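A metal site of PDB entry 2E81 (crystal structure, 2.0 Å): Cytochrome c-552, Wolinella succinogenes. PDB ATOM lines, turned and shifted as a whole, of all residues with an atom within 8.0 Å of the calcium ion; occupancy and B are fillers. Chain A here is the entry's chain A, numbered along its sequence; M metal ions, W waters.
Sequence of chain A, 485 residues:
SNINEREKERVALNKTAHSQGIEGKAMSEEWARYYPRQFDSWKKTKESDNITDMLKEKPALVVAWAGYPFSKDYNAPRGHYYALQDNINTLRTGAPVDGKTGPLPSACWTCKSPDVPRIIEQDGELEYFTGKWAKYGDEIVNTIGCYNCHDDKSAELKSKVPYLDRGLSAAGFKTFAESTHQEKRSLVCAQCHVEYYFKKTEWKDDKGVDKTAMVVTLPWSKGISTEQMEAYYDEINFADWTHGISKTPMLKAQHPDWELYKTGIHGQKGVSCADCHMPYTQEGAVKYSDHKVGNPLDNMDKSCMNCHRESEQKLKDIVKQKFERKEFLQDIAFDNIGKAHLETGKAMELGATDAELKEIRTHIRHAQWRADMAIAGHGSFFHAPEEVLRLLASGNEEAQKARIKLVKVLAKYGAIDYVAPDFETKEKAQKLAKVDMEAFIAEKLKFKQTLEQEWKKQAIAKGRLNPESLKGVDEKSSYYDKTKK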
ATOM      1  N   TYR A  68      -9.770  13.553 -22.286  1.00  0.00           N
ATOM      2  CA  TYR A  68      -9.319  12.160 -22.218  1.00  0.00           C
ATOM      3  C   TYR A  68     -10.375  11.283 -22.917  1.00  0.00           C
ATOM      4  O   TYR A  68     -11.556  11.628 -22.943  1.00  0.00           O
ATOM      5  CB  TYR A  68      -9.148  11.764 -20.754  1.00  0.00           C
ATOM      6  CG  TYR A  68      -8.250  10.570 -20.479  1.00  0.00           C
ATOM      7  CD1 TYR A  68      -6.924  10.553 -20.895  1.00  0.00           C
ATOM      8  CD2 TYR A  68      -8.733   9.466 -19.766  1.00  0.00           C
ATOM      9  CE1 TYR A  68      -6.085   9.462 -20.609  1.00  0.00           C
ATOM     10  CE2 TYR A  68      -7.907   8.378 -19.474  1.00  0.00           C
ATOM     11  CZ  TYR A  68      -6.587   8.391 -19.901  1.00  0.00           C
ATOM     12  OH  TYR A  68      -5.782   7.315 -19.611  1.00  0.00           O
ATOM     13  N   VAL A 194      -6.815  -4.757 -12.129  1.00  0.00           N
ATOM     14  CA  VAL A 194      -5.925  -3.912 -11.344  1.00  0.00           C
ATOM     15  C   VAL A 194      -5.723  -2.564 -12.035  1.00  0.00           C
ATOM     16  O   VAL A 194      -6.041  -2.409 -13.206  1.00  0.00           O
ATOM     17  CB  VAL A 194      -4.545  -4.569 -11.151  1.00  0.00           C
ATOM     18  CG1 VAL A 194      -4.662  -5.781 -10.250  1.00  0.00           C
ATOM     19  CG2 VAL A 194      -3.972  -4.968 -12.512  1.00  0.00           C
ATOM     20  N   GLU A 195      -5.186  -1.605 -11.287  1.00  0.00           N
ATOM     21  CA  GLU A 195      -4.883  -0.277 -11.806  1.00  0.00           C
ATOM     22  C   GLU A 195      -3.525  -0.399 -12.503  1.00  0.00           C
ATOM     23  O   GLU A 195      -2.674  -1.189 -12.088  1.00  0.00           O
ATOM     24  CB  GLU A 195      -4.844   0.727 -10.650  1.00  0.00           C
ATOM     25  CG  GLU A 195      -3.778   1.818 -10.743  1.00  0.00           C
ATOM     26  CD  GLU A 195      -4.015   2.817 -11.863  1.00  0.00           C
ATOM     27  OE1 GLU A 195      -5.102   2.806 -12.476  1.00  0.00           O
ATOM     28  OE2 GLU A 195      -3.113   3.628 -12.110  1.00  0.00           O
ATOM     29  N   TYR A 196      -3.325   0.382 -13.555  1.00  0.00           N
ATOM     30  CA  TYR A 196      -2.074   0.330 -14.307  1.00  0.00           C
ATOM     31  C   TYR A 196      -1.865   1.641 -15.063  1.00  0.00           C
ATOM     32  O   TYR A 196      -2.732   2.512 -15.082  1.00  0.00           O
ATOM     33  CB  TYR A 196      -2.161  -0.785 -15.349  1.00  0.00           C
ATOM     34  CG  TYR A 196      -3.088  -0.387 -16.489  1.00  0.00           C
ATOM     35  CD1 TYR A 196      -4.485  -0.463 -16.345  1.00  0.00           C
ATOM     36  CD2 TYR A 196      -2.589   0.163 -17.660  1.00  0.00           C
ATOM     37  CE1 TYR A 196      -5.343   0.026 -17.337  1.00  0.00           C
ATOM     38  CE2 TYR A 196      -3.435   0.650 -18.658  1.00  0.00           C
ATOM     39  CZ  TYR A 196      -4.798   0.586 -18.492  1.00  0.00           C
ATOM     40  OH  TYR A 196      -5.620   1.107 -19.467  1.00  0.00           O
ATOM     41  N   TYR A 197      -0.696   1.753 -15.697  1.00  0.00           N
ATOM     42  CA  TYR A 197      -0.382   2.902 -16.552  1.00  0.00           C
ATOM     43  C   TYR A 197       0.585   2.390 -17.612  1.00  0.00           C
ATOM     44  O   TYR A 197       1.217   1.348 -17.427  1.00  0.00           O
ATOM     45  CB  TYR A 197       0.233   4.072 -15.755  1.00  0.00           C
ATOM     46  CG  TYR A 197       1.696   3.936 -15.391  1.00  0.00           C
ATOM     47  CD1 TYR A 197       2.096   3.163 -14.292  1.00  0.00           C
ATOM     48  CD2 TYR A 197       2.679   4.608 -16.113  1.00  0.00           C
ATOM     49  CE1 TYR A 197       3.439   3.082 -13.927  1.00  0.00           C
ATOM     50  CE2 TYR A 197       4.026   4.525 -15.757  1.00  0.00           C
ATOM     51  CZ  TYR A 197       4.395   3.763 -14.664  1.00  0.00           C
ATOM     52  OH  TYR A 197       5.717   3.686 -14.298  1.00  0.00           O
ATOM     53  N   PHE A 198       0.679   3.088 -18.750  1.00  0.00           N
ATOM     54  CA  PHE A 198       1.591   2.676 -19.807  1.00  0.00           C
ATOM     55  C   PHE A 198       2.909   3.406 -19.652  1.00  0.00           C
ATOM     56  O   PHE A 198       2.946   4.639 -19.646  1.00  0.00           O
ATOM     57  CB  PHE A 198       1.019   2.980 -21.198  1.00  0.00           C
ATOM     58  CG  PHE A 198      -0.242   2.237 -21.539  1.00  0.00           C
ATOM     59  CD1 PHE A 198      -0.458   0.938 -21.071  1.00  0.00           C
ATOM     60  CD2 PHE A 198      -1.199   2.809 -22.373  1.00  0.00           C
ATOM     61  CE1 PHE A 198      -1.594   0.229 -21.426  1.00  0.00           C
ATOM     62  CE2 PHE A 198      -2.339   2.107 -22.744  1.00  0.00           C
ATOM     63  CZ  PHE A 198      -2.536   0.817 -22.270  1.00  0.00           C
ATOM     64  N   THR A 217       2.243  -1.276 -16.758  1.00  0.00           N
ATOM     65  CA  THR A 217       2.987  -1.263 -15.514  1.00  0.00           C
ATOM     66  C   THR A 217       2.074  -1.025 -14.326  1.00  0.00           C
ATOM     67  O   THR A 217       1.258  -0.116 -14.335  1.00  0.00           O
ATOM     68  CB  THR A 217       4.057  -0.134 -15.538  1.00  0.00           C
ATOM     69  OG1 THR A 217       4.916  -0.321 -16.674  1.00  0.00           O
ATOM     70  CG2 THR A 217       4.886  -0.144 -14.263  1.00  0.00           C
ATOM     71  N   PRO A 219       1.544   0.388 -10.820  1.00  0.00           N
ATOM     72  CA  PRO A 219       2.140   1.412  -9.953  1.00  0.00           C
ATOM     73  C   PRO A 219       2.195   0.995  -8.499  1.00  0.00           C
ATOM     74  O   PRO A 219       1.739   1.726  -7.616  1.00  0.00           O
ATOM     75  CB  PRO A 219       1.204   2.595 -10.163  1.00  0.00           C
ATOM     76  CG  PRO A 219      -0.132   1.901 -10.224  1.00  0.00           C
ATOM     77  CD  PRO A 219       0.153   0.722 -11.146  1.00  0.00           C
ATOM     78  N   MET A 229       0.100   4.738  -4.235  1.00  0.00           N
ATOM     79  CA  MET A 229       0.120   4.824  -5.693  1.00  0.00           C
ATOM     80  C   MET A 229       0.197   6.286  -6.111  1.00  0.00           C
ATOM     81  O   MET A 229       0.855   6.627  -7.096  1.00  0.00           O
ATOM     82  CB  MET A 229      -1.137   4.165  -6.272  1.00  0.00           C
ATOM     83  CG  MET A 229      -1.123   2.636  -6.201  1.00  0.00           C
ATOM     84  SD  MET A 229      -2.486   1.882  -7.122  1.00  0.00           S
ATOM     85  CE  MET A 229      -3.549   1.346  -5.821  1.00  0.00           C
ATOM     86  N   TYR A 233       3.054   8.043  -8.555  1.00  0.00           N
ATOM     87  CA  TYR A 233       2.864   8.866  -9.738  1.00  0.00           C
ATOM     88  C   TYR A 233       3.458  10.260  -9.580  1.00  0.00           C
ATOM     89  O   TYR A 233       4.073  10.784 -10.514  1.00  0.00           O
ATOM     90  CB  TYR A 233       1.367   8.971 -10.073  1.00  0.00           C
ATOM     91  CG  TYR A 233       0.803   7.712 -10.709  1.00  0.00           C
ATOM     92  CD1 TYR A 233       1.333   7.218 -11.891  1.00  0.00           C
ATOM     93  CD2 TYR A 233      -0.270   7.024 -10.132  1.00  0.00           C
ATOM     94  CE1 TYR A 233       0.813   6.085 -12.501  1.00  0.00           C
ATOM     95  CE2 TYR A 233      -0.803   5.884 -10.735  1.00  0.00           C
ATOM     96  CZ  TYR A 233      -0.249   5.416 -11.926  1.00  0.00           C
ATOM     97  OH  TYR A 233      -0.749   4.293 -12.530  1.00  0.00           O
ATOM     98  N   PHE A 238       4.212  12.012 -13.189  1.00  0.00           N
ATOM     99  CA  PHE A 238       3.429  11.397 -14.246  1.00  0.00           C
ATOM    100  C   PHE A 238       2.024  11.978 -14.382  1.00  0.00           C
ATOM    101  O   PHE A 238       1.389  12.353 -13.388  1.00  0.00           O
ATOM    102  CB  PHE A 238       3.319   9.892 -14.009  1.00  0.00           C
ATOM    103  CG  PHE A 238       2.633   9.139 -15.119  1.00  0.00           C
ATOM    104  CD1 PHE A 238       3.323   8.838 -16.291  1.00  0.00           C
ATOM    105  CD2 PHE A 238       1.309   8.749 -14.996  1.00  0.00           C
ATOM    106  CE1 PHE A 238       2.695   8.168 -17.334  1.00  0.00           C
ATOM    107  CE2 PHE A 238       0.667   8.072 -16.031  1.00  0.00           C
ATOM    108  CZ  PHE A 238       1.358   7.780 -17.206  1.00  0.00           C
ATOM    109  N   ASP A 240      -1.582  11.226 -16.957  1.00  0.00           N
ATOM    110  CA  ASP A 240      -2.196  10.463 -18.033  1.00  0.00           C
ATOM    111  C   ASP A 240      -2.664  11.434 -19.119  1.00  0.00           C
ATOM    112  O   ASP A 240      -2.689  11.087 -20.298  1.00  0.00           O
ATOM    113  CB  ASP A 240      -3.365   9.633 -17.488  1.00  0.00           C
ATOM    114  CG  ASP A 240      -2.903   8.387 -16.750  1.00  0.00           C
ATOM    115  OD1 ASP A 240      -2.353   7.491 -17.421  1.00  0.00           O
ATOM    116  OD2 ASP A 240      -3.078   8.304 -15.516  1.00  0.00           O
ATOM    117  N   TRP A 241      -3.006  12.647 -18.704  1.00  0.00           N
ATOM    118  CA  TRP A 241      -3.438  13.672 -19.644  1.00  0.00           C
ATOM    119  C   TRP A 241      -3.555  15.030 -18.964  1.00  0.00           C
ATOM    120  O   TRP A 241      -3.618  15.119 -17.735  1.00  0.00           O
ATOM    121  CB  TRP A 241      -4.785  13.266 -20.292  1.00  0.00           C
ATOM    122  CG  TRP A 241      -6.034  13.659 -19.540  1.00  0.00           C
ATOM    123  CD1 TRP A 241      -6.868  14.712 -19.813  1.00  0.00           C
ATOM    124  CD2 TRP A 241      -6.614  12.983 -18.410  1.00  0.00           C
ATOM    125  NE1 TRP A 241      -7.916  14.744 -18.925  1.00  0.00           N
ATOM    126  CE2 TRP A 241      -7.789  13.693 -18.060  1.00  0.00           C
ATOM    127  CE3 TRP A 241      -6.253  11.856 -17.661  1.00  0.00           C
ATOM    128  CZ2 TRP A 241      -8.606  13.300 -16.980  1.00  0.00           C
ATOM    129  CZ3 TRP A 241      -7.066  11.471 -16.592  1.00  0.00           C
ATOM    130  CH2 TRP A 241      -8.230  12.203 -16.267  1.00  0.00           C
ATOM    131  N   LEU A 251      -4.506  12.139 -13.340  1.00  0.00           N
ATOM    132  CA  LEU A 251      -4.192  10.733 -13.179  1.00  0.00           C
ATOM    133  C   LEU A 251      -5.508   9.980 -13.338  1.00  0.00           C
ATOM    134  O   LEU A 251      -6.519  10.360 -12.741  1.00  0.00           O
ATOM    135  CB  LEU A 251      -3.631  10.451 -11.789  1.00  0.00           C
ATOM    136  CG  LEU A 251      -2.231  10.971 -11.446  1.00  0.00           C
ATOM    137  CD1 LEU A 251      -1.882  10.566 -10.017  1.00  0.00           C
ATOM    138  CD2 LEU A 251      -1.215  10.391 -12.420  1.00  0.00           C
ATOM    139  N   LYS A 252      -5.495   8.932 -14.155  1.00  0.00           N
ATOM    140  CA  LYS A 252      -6.697   8.139 -14.378  1.00  0.00           C
ATOM    141  C   LYS A 252      -6.633   6.835 -13.599  1.00  0.00           C
ATOM    142  O   LYS A 252      -5.657   6.095 -13.709  1.00  0.00           O
ATOM    143  CB  LYS A 252      -6.855   7.793 -15.860  1.00  0.00           C
ATOM    144  CG  LYS A 252      -8.122   7.024 -16.185  1.00  0.00           C
ATOM    145  CD  LYS A 252      -9.348   7.933 -16.175  1.00  0.00           C
ATOM    146  CE  LYS A 252     -10.649   7.151 -16.319  1.00  0.00           C
ATOM    147  NZ  LYS A 252     -11.010   6.409 -15.066  1.00  0.00           N
ATOM    148  N   ALA A 253      -7.662   6.559 -12.812  1.00  0.00           N
ATOM    149  CA  ALA A 253      -7.688   5.306 -12.075  1.00  0.00           C
ATOM    150  C   ALA A 253      -8.447   4.312 -12.940  1.00  0.00           C
ATOM    151  O   ALA A 253      -9.480   4.654 -13.523  1.00  0.00           O
ATOM    152  CB  ALA A 253      -8.431   5.485 -10.753  1.00  0.00           C
ATOM    153  N   GLN A 254      -7.933   3.100 -13.069  1.00  0.00           N
ATOM    154  CA  GLN A 254      -8.626   2.097 -13.859  1.00  0.00           C
ATOM    155  C   GLN A 254      -8.833   0.823 -13.079  1.00  0.00           C
ATOM    156  O   GLN A 254      -7.885   0.185 -12.634  1.00  0.00           O
ATOM    157  CB  GLN A 254      -7.882   1.777 -15.160  1.00  0.00           C
ATOM    158  CG  GLN A 254      -7.982   2.870 -16.218  1.00  0.00           C
ATOM    159  CD  GLN A 254      -6.639   3.506 -16.508  1.00  0.00           C
ATOM    160  OE1 GLN A 254      -5.848   3.739 -15.603  1.00  0.00           O
ATOM    161  NE2 GLN A 254      -6.393   3.810 -17.779  1.00  0.00           N
ATOM    162  N   HIS A 255     -10.111   0.487 -12.886  1.00  0.00           N
ATOM    163  CA  HIS A 255     -10.510  -0.734 -12.191  1.00  0.00           C
ATOM    164  C   HIS A 255      -9.478  -1.371 -11.250  1.00  0.00           C
ATOM    165  O   HIS A 255      -8.918  -2.426 -11.564  1.00  0.00           O
ATOM    166  CB  HIS A 255     -10.955  -1.756 -13.231  1.00  0.00           C
ATOM    167  CG  HIS A 255     -10.042  -1.817 -14.416  1.00  0.00           C
ATOM    168  ND1 HIS A 255      -8.708  -2.160 -14.314  1.00  0.00           N
ATOM    169  CD2 HIS A 255     -10.259  -1.521 -15.722  1.00  0.00           C
ATOM    170  CE1 HIS A 255      -8.137  -2.060 -15.511  1.00  0.00           C
ATOM    171  NE2 HIS A 255      -9.061  -1.676 -16.376  1.00  0.00           N
ATOM    172  N   TRP A 369      -7.949  11.700  -8.285  1.00  0.00           N
ATOM    173  CA  TRP A 369      -7.252  10.427  -8.206  1.00  0.00           C
ATOM    174  C   TRP A 369      -7.892   9.572  -7.115  1.00  0.00           C
ATOM    175  O   TRP A 369      -8.141   8.387  -7.314  1.00  0.00           O
ATOM    176  CB  TRP A 369      -5.768  10.620  -7.887  1.00  0.00           C
ATOM    177  CG  TRP A 369      -5.082   9.327  -7.525  1.00  0.00           C
ATOM    178  CD1 TRP A 369      -4.579   8.976  -6.307  1.00  0.00           C
ATOM    179  CD2 TRP A 369      -4.855   8.202  -8.386  1.00  0.00           C
ATOM    180  NE1 TRP A 369      -4.059   7.704  -6.348  1.00  0.00           N
ATOM    181  CE2 TRP A 369      -4.220   7.204  -7.616  1.00  0.00           C
ATOM    182  CE3 TRP A 369      -5.132   7.932  -9.739  1.00  0.00           C
ATOM    183  CZ2 TRP A 369      -3.852   5.960  -8.146  1.00  0.00           C
ATOM    184  CZ3 TRP A 369      -4.766   6.700 -10.262  1.00  0.00           C
ATOM    185  CH2 TRP A 369      -4.131   5.730  -9.466  1.00  0.00           C
ATOM    186  N   ASP A 372     -11.686   8.732  -8.066  1.00  0.00           N
ATOM    187  CA  ASP A 372     -11.732   7.807  -9.204  1.00  0.00           C
ATOM    188  C   ASP A 372     -11.304   6.427  -8.721  1.00  0.00           C
ATOM    189  O   ASP A 372     -11.913   5.417  -9.091  1.00  0.00           O
ATOM    190  CB  ASP A 372     -10.808   8.310 -10.328  1.00  0.00           C
ATOM    191  CG  ASP A 372     -11.170   7.727 -11.690  1.00  0.00           C
ATOM    192  OD1 ASP A 372     -12.181   7.014 -11.800  1.00  0.00           O
ATOM    193  OD2 ASP A 372     -10.429   8.008 -12.667  1.00  0.00           O
ATOM    194  N   MET A 373     -10.254   6.373  -7.892  1.00  0.00           N
ATOM    195  CA  MET A 373      -9.783   5.097  -7.355  1.00  0.00           C
ATOM    196  C   MET A 373     -10.889   4.419  -6.547  1.00  0.00           C
ATOM    197  O   MET A 373     -10.970   3.202  -6.475  1.00  0.00           O
ATOM    198  CB  MET A 373      -8.575   5.297  -6.434  1.00  0.00           C
ATOM    199  CG  MET A 373      -7.229   5.305  -7.153  1.00  0.00           C
ATOM    200  SD  MET A 373      -6.841   3.685  -7.888  1.00  0.00           S
ATOM    201  CE  MET A 373      -6.524   2.728  -6.442  1.00  0.00           C
HETATM  202 CA    CA M   1      -4.031   4.480 -14.239  1.00  0.00          CA
HETATM  203  O   HOH W   1      -3.518   5.125 -16.547  1.00  0.00           O
HETATM  204  O   HOH W   2      -2.413   6.244 -14.009  1.00  0.00           O
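Water W2 lies within hydrogen-bond range of OD2 of Asp 240 (2.6 Å) and OH of Tyr 233 (3.0 Å).
Water W1 lies within hydrogen-bond range of the side-chain carboxylate of Asp 240 (2.8 Å) and the side-chain amide nitrogen of Gln 254 (3.4 Å).
The side-chain carboxylate (OD2) of Asp 240 is in hydrogen-bond range of the backbone NH (N) of Lys 252 (2.8 Å).
NZ of Lys 252 is in salt-bridge range of OD2 of Asp 372 (2.9 Å).
The side-chain carboxylate of Glu 195 sits close to the side-chain hydroxyl of Tyr 233 (2.5 Å).
O of Tyr 233 is in hydrogen-bond range of N of Phe 238 (2.9 Å).
O of Lys 252 binds the calcium ion (2.4 Å).
The calcium ion is bound by OE1 of Gln 254 (2.4 Å).
Water W2 binds the calcium ion, 2.4 Å away.
Water W1 binds the calcium ion (2.5 Å).
OE2 of Glu 195 is bound to the calcium ion, 2.5 Å away.
The backbone carbonyl oxygen (O) of Tyr 196 binds the calcium ion (2.5 Å).
The side-chain carboxylate (OE1) of Glu 195 is bound to the calcium ion, 2.7 Å away.
The calcium ion has seven donor atoms within binding distance.
Tyr 233 touches the calcium ion.
Of the 21 residues printed, 5 come within 4 Å of the calcium ion.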
